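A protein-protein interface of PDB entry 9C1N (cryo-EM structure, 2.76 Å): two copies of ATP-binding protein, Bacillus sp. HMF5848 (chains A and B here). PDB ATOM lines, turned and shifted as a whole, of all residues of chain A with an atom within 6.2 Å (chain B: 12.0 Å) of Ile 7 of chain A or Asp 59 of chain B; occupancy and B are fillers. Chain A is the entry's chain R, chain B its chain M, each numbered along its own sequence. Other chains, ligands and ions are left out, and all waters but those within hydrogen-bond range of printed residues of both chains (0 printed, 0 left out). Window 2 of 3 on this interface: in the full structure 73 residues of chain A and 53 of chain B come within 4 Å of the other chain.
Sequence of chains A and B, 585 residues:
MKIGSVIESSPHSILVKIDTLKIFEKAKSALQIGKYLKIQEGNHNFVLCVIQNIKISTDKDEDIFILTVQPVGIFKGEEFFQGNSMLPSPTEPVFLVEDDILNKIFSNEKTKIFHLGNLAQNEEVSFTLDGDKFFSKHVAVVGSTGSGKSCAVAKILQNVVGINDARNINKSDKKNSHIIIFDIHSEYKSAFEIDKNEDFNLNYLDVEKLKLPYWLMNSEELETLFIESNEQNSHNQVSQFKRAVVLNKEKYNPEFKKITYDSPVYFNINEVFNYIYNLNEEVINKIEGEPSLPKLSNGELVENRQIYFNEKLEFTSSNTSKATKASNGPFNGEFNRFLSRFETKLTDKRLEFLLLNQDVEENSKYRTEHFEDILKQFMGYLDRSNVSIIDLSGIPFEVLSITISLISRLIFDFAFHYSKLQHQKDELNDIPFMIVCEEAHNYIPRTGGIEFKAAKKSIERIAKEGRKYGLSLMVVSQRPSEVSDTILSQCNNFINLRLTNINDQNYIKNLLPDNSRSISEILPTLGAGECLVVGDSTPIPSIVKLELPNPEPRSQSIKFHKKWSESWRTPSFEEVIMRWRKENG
The backbone NH (N) of Ile 66 of chain B lies within hydrogen-bond range of the backbone carbonyl oxygen (O) of Lys 55 of chain B, at 3.1 Å. The backbone carbonyl oxygen of Ser 57 of chain B lies close to the backbone carbonyl oxygen of Glu 62 of chain B, 2.7 Å away. The backbone carbonyl oxygen of Ser 57 of chain B lies within hydrogen-bond range of the backbone NH of Ile 64 of chain B (2.7 Å). OD1 of Asp 63 of chain B sits close to OG1 of Thr 58 of chain B (3.5 Å). The backbone NH (N) of Ile 7 of chain A lies within hydrogen-bond range of the backbone carbonyl oxygen (O) of Leu 15 of chain A (2.9 Å). O of Glu 8 of chain A lies within hydrogen-bond range of N of Leu 15 of chain A, 2.7 Å away.
Ser 5 of chain A touches none of the printed residues of chain B. No residue of chain B comes within 4 Å of Val 6 of chain A. Glu 8 of chain A touches just these residues of chain B: Lys 55, Ile 56 and Ser 57. Ser 9 of chain A touches two residues of chain B. Ile 14 of chain A touches none of the printed residues of chain B. No residue of chain B comes within 4 Å of Leu 15 of chain A. No residue of chain B comes within 4 Å of Val 16 of chain A. No residue of chain B comes within 4 Å of Lys 17 of chain A. No residue of chain B comes within 4 Å of Ile 66 of chain A. Of the printed residues of chain B, Pro 90 of chain A touches Ile 56 and Thr 58. Printed residues of chain A within 4 Å of Lys 55 of chain B: Glu 8 and Ser 9. Printed residues of chain A within 4 Å of Ile 56 of chain B: Glu 8 (3.4 Å), Ser 9 (3.0 Å) and Pro 90 (3.9 Å). Of the printed residues of chain A, Ser 57 of chain B touches Ile 7 (3.8 Å) and Glu 8 (3.4 Å). Of the printed residues of chain A, Thr 58 of chain B touches Ile 7 (3.2 Å) and Pro 90 (3.1 Å). Of chain A, only Ile 7 (3.4 Å) comes within 4 Å of Asp 59 of chain B. The nearest residue of chain A that does not touch Asp 59 of chain B is Glu 8 of chain A (4.6 Å). The nearest printed residue of chain A that does not touch Ser 57 of chain B is Pro 90 of chain A (4.5 Å).
Printed residues of chain A that touch a printed residue of chain B: Ile 7, Glu 8, Ser 9 and Pro 90. Hydrophobic or aromatic side chains of chain A within 4 Å of the printed part of chain B: Ile 7 and Pro 90. Among the printed residues, Asp or Glu carboxylates within 4 Å of a Lys or Arg side-chain nitrogen of the other chain: Glu 8 of chain A with Lys 55 of chain B (3.1 Å).
Position printed for both chains: 66. Of the 10 pairs that touch across the chains among the printed residues, none has its exchanged pair printed and touching as well.
Ser 57 of chain B touches Ile 7 of chain A (CA to O, 3.8 Å). Ile 7 of chain A touches Asp 59 of chain B (CD1 to OD1, 3.4 Å). Ile 56 of chain B touches Glu 8 of chain A. Glu 8 of chain A touches Ser 57 of chain B. O of Ser 9 of chain A touches CA of Lys 55 of chain B (3.8 Å). Pro 90 of chain A touches Ile 56 of chain B. OG1 of Thr 58 of chain B touches CB of Pro 90 of chain A (3.1 Å).
The side-chain amino group (NZ) of Lys 55 of chain B lies within salt-bridge range of the side-chain carboxylate (OE2) of Glu 8 of chain A (3.1 Å). The backbone carbonyl oxygen (O) of Ile 56 of chain B lies within hydrogen-bond range of the backbone NH (N) of Ser 9 of chain A (3.0 Å). N of Thr 58 of chain B lies within hydrogen-bond range of O of Ile 7 of chain A (3.2 Å).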
ATOM      1  N   SER A   5      -2.854  31.330 -15.392  1.00  0.00           N
ATOM      2  CA  SER A   5      -3.101  29.936 -15.731  1.00  0.00           C
ATOM      3  C   SER A   5      -3.768  29.866 -17.097  1.00  0.00           C
ATOM      4  O   SER A   5      -4.335  30.846 -17.585  1.00  0.00           O
ATOM      5  CB  SER A   5      -3.970  29.245 -14.673  1.00  0.00           C
ATOM      6  OG  SER A   5      -5.242  29.861 -14.576  1.00  0.00           O
ATOM      7  N   VAL A   6      -3.698  28.686 -17.705  1.00  0.00           N
ATOM      8  CA  VAL A   6      -4.236  28.458 -19.042  1.00  0.00           C
ATOM      9  C   VAL A   6      -5.673  27.970 -18.926  1.00  0.00           C
ATOM     10  O   VAL A   6      -5.969  27.055 -18.148  1.00  0.00           O
ATOM     11  CB  VAL A   6      -3.372  27.449 -19.815  1.00  0.00           C
ATOM     12  CG1 VAL A   6      -4.005  27.120 -21.157  1.00  0.00           C
ATOM     13  CG2 VAL A   6      -1.966  27.989 -19.997  1.00  0.00           C
ATOM     14  N   ILE A   7      -6.571  28.581 -19.697  1.00  0.00           N
ATOM     15  CA  ILE A   7      -7.976  28.200 -19.691  1.00  0.00           C
ATOM     16  C   ILE A   7      -8.425  27.561 -21.000  1.00  0.00           C
ATOM     17  O   ILE A   7      -9.454  26.867 -21.006  1.00  0.00           O
ATOM     18  CB  ILE A   7      -8.880  29.402 -19.352  1.00  0.00           C
ATOM     19  CG1 ILE A   7      -8.695  30.520 -20.379  1.00  0.00           C
ATOM     20  CG2 ILE A   7      -8.592  29.903 -17.946  1.00  0.00           C
ATOM     21  CD1 ILE A   7      -9.844  31.503 -20.426  1.00  0.00           C
ATOM     22  N   GLU A   8      -7.704  27.766 -22.101  1.00  0.00           N
ATOM     23  CA  GLU A   8      -8.063  27.145 -23.370  1.00  0.00           C
ATOM     24  C   GLU A   8      -6.830  27.130 -24.260  1.00  0.00           C
ATOM     25  O   GLU A   8      -6.155  28.153 -24.399  1.00  0.00           O
ATOM     26  CB  GLU A   8      -9.212  27.901 -24.053  1.00  0.00           C
ATOM     27  CG  GLU A   8      -9.810  27.193 -25.270  1.00  0.00           C
ATOM     28  CD  GLU A   8      -9.032  27.432 -26.550  1.00  0.00           C
ATOM     29  OE1 GLU A   8      -8.399  28.498 -26.676  1.00  0.00           O
ATOM     30  OE2 GLU A   8      -9.056  26.551 -27.435  1.00  0.00           O
ATOM     31  N   SER A   9      -6.542  25.978 -24.861  1.00  0.00           N
ATOM     32  CA  SER A   9      -5.404  25.832 -25.756  1.00  0.00           C
ATOM     33  C   SER A   9      -5.878  25.292 -27.097  1.00  0.00           C
ATOM     34  O   SER A   9      -6.539  24.251 -27.156  1.00  0.00           O
ATOM     35  CB  SER A   9      -4.337  24.908 -25.158  1.00  0.00           C
ATOM     36  OG  SER A   9      -3.817  25.443 -23.953  1.00  0.00           O
ATOM     37  N   ILE A  14      -3.725  30.411 -27.489  1.00  0.00           N
ATOM     38  CA  ILE A  14      -3.793  29.919 -26.119  1.00  0.00           C
ATOM     39  C   ILE A  14      -4.314  31.049 -25.242  1.00  0.00           C
ATOM     40  O   ILE A  14      -3.752  32.149 -25.248  1.00  0.00           O
ATOM     41  CB  ILE A  14      -2.422  29.428 -25.614  1.00  0.00           C
ATOM     42  CG1 ILE A  14      -2.028  28.121 -26.302  1.00  0.00           C
ATOM     43  CG2 ILE A  14      -2.437  29.253 -24.102  1.00  0.00           C
ATOM     44  CD1 ILE A  14      -0.532  27.915 -26.415  1.00  0.00           C
ATOM     45  N   LEU A  15      -5.382  30.781 -24.495  1.00  0.00           N
ATOM     46  CA  LEU A  15      -5.987  31.771 -23.612  1.00  0.00           C
ATOM     47  C   LEU A  15      -5.486  31.579 -22.186  1.00  0.00           C
ATOM     48  O   LEU A  15      -5.446  30.453 -21.680  1.00  0.00           O
ATOM     49  CB  LEU A  15      -7.514  31.701 -23.660  1.00  0.00           C
ATOM     50  CG  LEU A  15      -8.209  32.330 -24.876  1.00  0.00           C
ATOM     51  CD1 LEU A  15      -8.011  31.530 -26.151  1.00  0.00           C
ATOM     52  CD2 LEU A  15      -9.692  32.521 -24.591  1.00  0.00           C
ATOM     53  N   VAL A  16      -5.107  32.685 -21.546  1.00  0.00           N
ATOM     54  CA  VAL A  16      -4.503  32.680 -20.221  1.00  0.00           C
ATOM     55  C   VAL A  16      -5.301  33.607 -19.313  1.00  0.00           C
ATOM     56  O   VAL A  16      -5.659  34.722 -19.710  1.00  0.00           O
ATOM     57  CB  VAL A  16      -3.020  33.108 -20.278  1.00  0.00           C
ATOM     58  CG1 VAL A  16      -2.468  33.341 -18.878  1.00  0.00           C
ATOM     59  CG2 VAL A  16      -2.194  32.068 -21.020  1.00  0.00           C
ATOM     60  N   LYS A  17      -5.581  33.143 -18.099  1.00  0.00           N
ATOM     61  CA  LYS A  17      -6.344  33.894 -17.110  1.00  0.00           C
ATOM     62  C   LYS A  17      -5.415  34.404 -16.018  1.00  0.00           C
ATOM     63  O   LYS A  17      -4.638  33.630 -15.447  1.00  0.00           O
ATOM     64  CB  LYS A  17      -7.444  33.024 -16.499  1.00  0.00           C
ATOM     65  CG  LYS A  17      -8.329  33.743 -15.497  1.00  0.00           C
ATOM     66  CD  LYS A  17      -9.459  32.843 -15.024  1.00  0.00           C
ATOM     67  CE  LYS A  17     -10.259  33.502 -13.914  1.00  0.00           C
ATOM     68  NZ  LYS A  17     -10.982  34.707 -14.397  1.00  0.00           N
ATOM     69  N   ILE A  66      -8.194  38.249 -19.256  1.00  0.00           N
ATOM     70  CA  ILE A  66      -7.998  37.207 -20.258  1.00  0.00           C
ATOM     71  C   ILE A  66      -6.891  37.630 -21.214  1.00  0.00           C
ATOM     72  O   ILE A  66      -6.894  38.757 -21.721  1.00  0.00           O
ATOM     73  CB  ILE A  66      -9.301  36.910 -21.022  1.00  0.00           C
ATOM     74  CG1 ILE A  66     -10.359  36.361 -20.062  1.00  0.00           C
ATOM     75  CG2 ILE A  66      -9.051  35.924 -22.152  1.00  0.00           C
ATOM     76  CD1 ILE A  66      -9.966  35.059 -19.402  1.00  0.00           C
ATOM     77  N   PRO A  90      -4.740  22.673 -20.040  1.00  0.00           N
ATOM     78  CA  PRO A  90      -5.342  23.763 -19.267  1.00  0.00           C
ATOM     79  C   PRO A  90      -4.868  23.760 -17.821  1.00  0.00           C
ATOM     80  O   PRO A  90      -4.391  22.755 -17.290  1.00  0.00           O
ATOM     81  CB  PRO A  90      -6.843  23.477 -19.358  1.00  0.00           C
ATOM     82  CG  PRO A  90      -6.992  22.667 -20.602  1.00  0.00           C
ATOM     83  CD  PRO A  90      -5.761  21.817 -20.666  1.00  0.00           C
ATOM     84  N   THR A  91      -4.997  24.930 -17.192  1.00  0.00           N
ATOM     85  CA  THR A  91      -4.593  25.186 -15.807  1.00  0.00           C
ATOM     86  C   THR A  91      -3.088  25.039 -15.600  1.00  0.00           C
ATOM     87  O   THR A  91      -2.625  24.909 -14.461  1.00  0.00           O
ATOM     88  CB  THR A  91      -5.351  24.294 -14.813  1.00  0.00           C
ATOM     89  OG1 THR A  91      -4.984  22.923 -15.005  1.00  0.00           O
ATOM     90  CG2 THR A  91      -6.853  24.441 -15.011  1.00  0.00           C
ATOM     91  N   LEU B  21      -7.850  13.196 -19.132  1.00  0.00           N
ATOM     92  CA  LEU B  21      -6.688  14.066 -19.292  1.00  0.00           C
ATOM     93  C   LEU B  21      -5.403  13.263 -19.456  1.00  0.00           C
ATOM     94  O   LEU B  21      -4.540  13.624 -20.267  1.00  0.00           O
ATOM     95  CB  LEU B  21      -6.579  15.015 -18.099  1.00  0.00           C
ATOM     96  CG  LEU B  21      -5.406  15.998 -18.114  1.00  0.00           C
ATOM     97  CD1 LEU B  21      -5.611  17.071 -19.167  1.00  0.00           C
ATOM     98  CD2 LEU B  21      -5.213  16.622 -16.738  1.00  0.00           C
ATOM     99  N   PHE B  24      -4.892  11.997 -22.932  1.00  0.00           N
ATOM    100  CA  PHE B  24      -4.437  13.078 -23.802  1.00  0.00           C
ATOM    101  C   PHE B  24      -2.958  13.374 -23.589  1.00  0.00           C
ATOM    102  O   PHE B  24      -2.218  13.598 -24.553  1.00  0.00           O
ATOM    103  CB  PHE B  24      -5.276  14.333 -23.561  1.00  0.00           C
ATOM    104  CG  PHE B  24      -4.751  15.557 -24.257  1.00  0.00           C
ATOM    105  CD1 PHE B  24      -4.767  15.646 -25.639  1.00  0.00           C
ATOM    106  CD2 PHE B  24      -4.241  16.620 -23.532  1.00  0.00           C
ATOM    107  CE1 PHE B  24      -4.284  16.770 -26.281  1.00  0.00           C
ATOM    108  CE2 PHE B  24      -3.758  17.746 -24.169  1.00  0.00           C
ATOM    109  CZ  PHE B  24      -3.779  17.821 -25.544  1.00  0.00           C
ATOM    110  N   ILE B  54      -7.813  20.875 -33.112  1.00  0.00           N
ATOM    111  CA  ILE B  54      -7.837  20.414 -31.730  1.00  0.00           C
ATOM    112  C   ILE B  54      -8.245  21.585 -30.849  1.00  0.00           C
ATOM    113  O   ILE B  54      -7.986  22.748 -31.173  1.00  0.00           O
ATOM    114  CB  ILE B  54      -6.471  19.837 -31.287  1.00  0.00           C
ATOM    115  CG1 ILE B  54      -5.855  18.993 -32.407  1.00  0.00           C
ATOM    116  CG2 ILE B  54      -6.617  19.010 -30.021  1.00  0.00           C
ATOM    117  CD1 ILE B  54      -4.405  18.626 -32.188  1.00  0.00           C
ATOM    118  N   LYS B  55      -8.900  21.274 -29.731  1.00  0.00           N
ATOM    119  CA  LYS B  55      -9.351  22.313 -28.809  1.00  0.00           C
ATOM    120  C   LYS B  55      -9.531  21.685 -27.435  1.00  0.00           C
ATOM    121  O   LYS B  55     -10.397  20.821 -27.260  1.00  0.00           O
ATOM    122  CB  LYS B  55     -10.647  22.950 -29.298  1.00  0.00           C
ATOM    123  CG  LYS B  55     -11.149  24.082 -28.418  1.00  0.00           C
ATOM    124  CD  LYS B  55     -12.380  24.746 -29.018  1.00  0.00           C
ATOM    125  CE  LYS B  55     -12.971  25.777 -28.069  1.00  0.00           C
ATOM    126  NZ  LYS B  55     -12.053  26.928 -27.859  1.00  0.00           N
ATOM    127  N   ILE B  56      -8.727  22.117 -26.469  1.00  0.00           N
ATOM    128  CA  ILE B  56      -8.841  21.671 -25.087  1.00  0.00           C
ATOM    129  C   ILE B  56      -9.270  22.866 -24.244  1.00  0.00           C
ATOM    130  O   ILE B  56      -8.628  23.924 -24.274  1.00  0.00           O
ATOM    131  CB  ILE B  56      -7.530  21.045 -24.581  1.00  0.00           C
ATOM    132  CG1 ILE B  56      -6.356  22.015 -24.711  1.00  0.00           C
ATOM    133  CG2 ILE B  56      -7.221  19.776 -25.358  1.00  0.00           C
ATOM    134  CD1 ILE B  56      -5.003  21.390 -24.425  1.00  0.00           C
ATOM    135  N   SER B  57     -10.372  22.710 -23.514  1.00  0.00           N
ATOM    136  CA  SER B  57     -10.965  23.809 -22.765  1.00  0.00           C
ATOM    137  C   SER B  57     -11.364  23.335 -21.377  1.00  0.00           C
ATOM    138  O   SER B  57     -11.900  22.235 -21.219  1.00  0.00           O
ATOM    139  CB  SER B  57     -12.189  24.383 -23.492  1.00  0.00           C
ATOM    140  OG  SER B  57     -11.923  24.574 -24.871  1.00  0.00           O
ATOM    141  N   THR B  58     -11.087  24.169 -20.377  1.00  0.00           N
ATOM    142  CA  THR B  58     -11.482  23.918 -18.992  1.00  0.00           C
ATOM    143  C   THR B  58     -12.043  25.200 -18.381  1.00  0.00           C
ATOM    144  O   THR B  58     -11.640  25.643 -17.304  1.00  0.00           O
ATOM    145  CB  THR B  58     -10.315  23.360 -18.177  1.00  0.00           C
ATOM    146  OG1 THR B  58      -9.685  22.307 -18.915  1.00  0.00           O
ATOM    147  CG2 THR B  58     -10.799  22.802 -16.843  1.00  0.00           C
ATOM    148  N   ASP B  59     -12.972  25.833 -19.091  1.00  0.00           N
ATOM    149  CA  ASP B  59     -13.641  27.014 -18.564  1.00  0.00           C
ATOM    150  C   ASP B  59     -14.758  26.596 -17.615  1.00  0.00           C
ATOM    151  O   ASP B  59     -15.619  25.786 -17.975  1.00  0.00           O
ATOM    152  CB  ASP B  59     -14.197  27.868 -19.703  1.00  0.00           C
ATOM    153  CG  ASP B  59     -13.110  28.588 -20.474  1.00  0.00           C
ATOM    154  OD1 ASP B  59     -12.263  29.250 -19.836  1.00  0.00           O
ATOM    155  OD2 ASP B  59     -13.100  28.495 -21.720  1.00  0.00           O
ATOM    156  N   LYS B  60     -14.733  27.148 -16.401  1.00  0.00           N
ATOM    157  CA  LYS B  60     -15.748  26.885 -15.378  1.00  0.00           C
ATOM    158  C   LYS B  60     -15.831  25.397 -15.038  1.00  0.00           C
ATOM    159  O   LYS B  60     -16.915  24.810 -14.969  1.00  0.00           O
ATOM    160  CB  LYS B  60     -17.113  27.430 -15.809  1.00  0.00           C
ATOM    161  CG  LYS B  60     -17.946  27.989 -14.668  1.00  0.00           C
ATOM    162  CD  LYS B  60     -19.305  28.461 -15.159  1.00  0.00           C
ATOM    163  CE  LYS B  60     -20.203  28.859 -14.000  1.00  0.00           C
ATOM    164  NZ  LYS B  60     -20.650  27.678 -13.212  1.00  0.00           N
ATOM    165  N   ASP B  61     -14.663  24.786 -14.819  1.00  0.00           N
ATOM    166  CA  ASP B  61     -14.556  23.394 -14.373  1.00  0.00           C
ATOM    167  C   ASP B  61     -15.270  22.439 -15.329  1.00  0.00           C
ATOM    168  O   ASP B  61     -16.080  21.604 -14.923  1.00  0.00           O
ATOM    169  CB  ASP B  61     -15.088  23.235 -12.946  1.00  0.00           C
ATOM    170  CG  ASP B  61     -14.109  23.726 -11.899  1.00  0.00           C
ATOM    171  OD1 ASP B  61     -12.887  23.555 -12.098  1.00  0.00           O
ATOM    172  OD2 ASP B  61     -14.560  24.284 -10.876  1.00  0.00           O
ATOM    173  N   GLU B  62     -14.957  22.566 -16.619  1.00  0.00           N
ATOM    174  CA  GLU B  62     -15.556  21.735 -17.665  1.00  0.00           C
ATOM    175  C   GLU B  62     -14.429  21.228 -18.564  1.00  0.00           C
ATOM    176  O   GLU B  62     -14.017  21.912 -19.503  1.00  0.00           O
ATOM    177  CB  GLU B  62     -16.606  22.520 -18.448  1.00  0.00           C
ATOM    178  CG  GLU B  62     -17.224  21.759 -19.610  1.00  0.00           C
ATOM    179  CD  GLU B  62     -18.484  21.014 -19.219  1.00  0.00           C
ATOM    180  OE1 GLU B  62     -18.818  20.994 -18.016  1.00  0.00           O
ATOM    181  OE2 GLU B  62     -19.144  20.447 -20.116  1.00  0.00           O
ATOM    182  N   ASP B  63     -13.935  20.025 -18.270  1.00  0.00           N
ATOM    183  CA  ASP B  63     -12.857  19.418 -19.046  1.00  0.00           C
ATOM    184  C   ASP B  63     -13.383  19.003 -20.416  1.00  0.00           C
ATOM    185  O   ASP B  63     -14.139  18.033 -20.530  1.00  0.00           O
ATOM    186  CB  ASP B  63     -12.282  18.218 -18.301  1.00  0.00           C
ATOM    187  CG  ASP B  63     -11.525  18.613 -17.049  1.00  0.00           C
ATOM    188  OD1 ASP B  63     -10.967  19.726 -17.017  1.00  0.00           O
ATOM    189  OD2 ASP B  63     -11.486  17.808 -16.094  1.00  0.00           O
ATOM    190  N   ILE B  64     -12.982  19.729 -21.457  1.00  0.00           N
ATOM    191  CA  ILE B  64     -13.394  19.447 -22.826  1.00  0.00           C
ATOM    192  C   ILE B  64     -12.151  19.208 -23.672  1.00  0.00           C
ATOM    193  O   ILE B  64     -11.225  20.026 -23.669  1.00  0.00           O
ATOM    194  CB  ILE B  64     -14.242  20.591 -23.412  1.00  0.00           C
ATOM    195  CG1 ILE B  64     -15.492  20.816 -22.563  1.00  0.00           C
ATOM    196  CG2 ILE B  64     -14.624  20.290 -24.850  1.00  0.00           C
ATOM    197  CD1 ILE B  64     -16.406  19.612 -22.496  1.00  0.00           C
ATOM    198  N   PHE B  65     -12.136  18.086 -24.391  1.00  0.00           N
ATOM    199  CA  PHE B  65     -11.070  17.747 -25.334  1.00  0.00           C
ATOM    200  C   PHE B  65     -11.752  17.248 -26.605  1.00  0.00           C
ATOM    201  O   PHE B  65     -12.096  16.066 -26.707  1.00  0.00           O
ATOM    202  CB  PHE B  65     -10.111  16.697 -24.769  1.00  0.00           C
ATOM    203  CG  PHE B  65      -9.675  16.951 -23.346  1.00  0.00           C
ATOM    204  CD1 PHE B  65     -10.521  16.688 -22.280  1.00  0.00           C
ATOM    205  CD2 PHE B  65      -8.413  17.453 -23.078  1.00  0.00           C
ATOM    206  CE1 PHE B  65     -10.117  16.923 -20.979  1.00  0.00           C
ATOM    207  CE2 PHE B  65      -8.005  17.690 -21.779  1.00  0.00           C
ATOM    208  CZ  PHE B  65      -8.857  17.424 -20.730  1.00  0.00           C
ATOM    209  N   ILE B  66     -11.946  18.144 -27.570  1.00  0.00           N
ATOM    210  CA  ILE B  66     -12.706  17.855 -28.780  1.00  0.00           C
ATOM    211  C   ILE B  66     -11.779  17.965 -29.981  1.00  0.00           C
ATOM    212  O   ILE B  66     -11.048  18.953 -30.121  1.00  0.00           O
ATOM    213  CB  ILE B  66     -13.912  18.802 -28.929  1.00  0.00           C
ATOM    214  CG1 ILE B  66     -15.003  18.434 -27.924  1.00  0.00           C
ATOM    215  CG2 ILE B  66     -14.457  18.764 -30.350  1.00  0.00           C
ATOM    216  CD1 ILE B  66     -16.310  19.167 -28.138  1.00  0.00           C
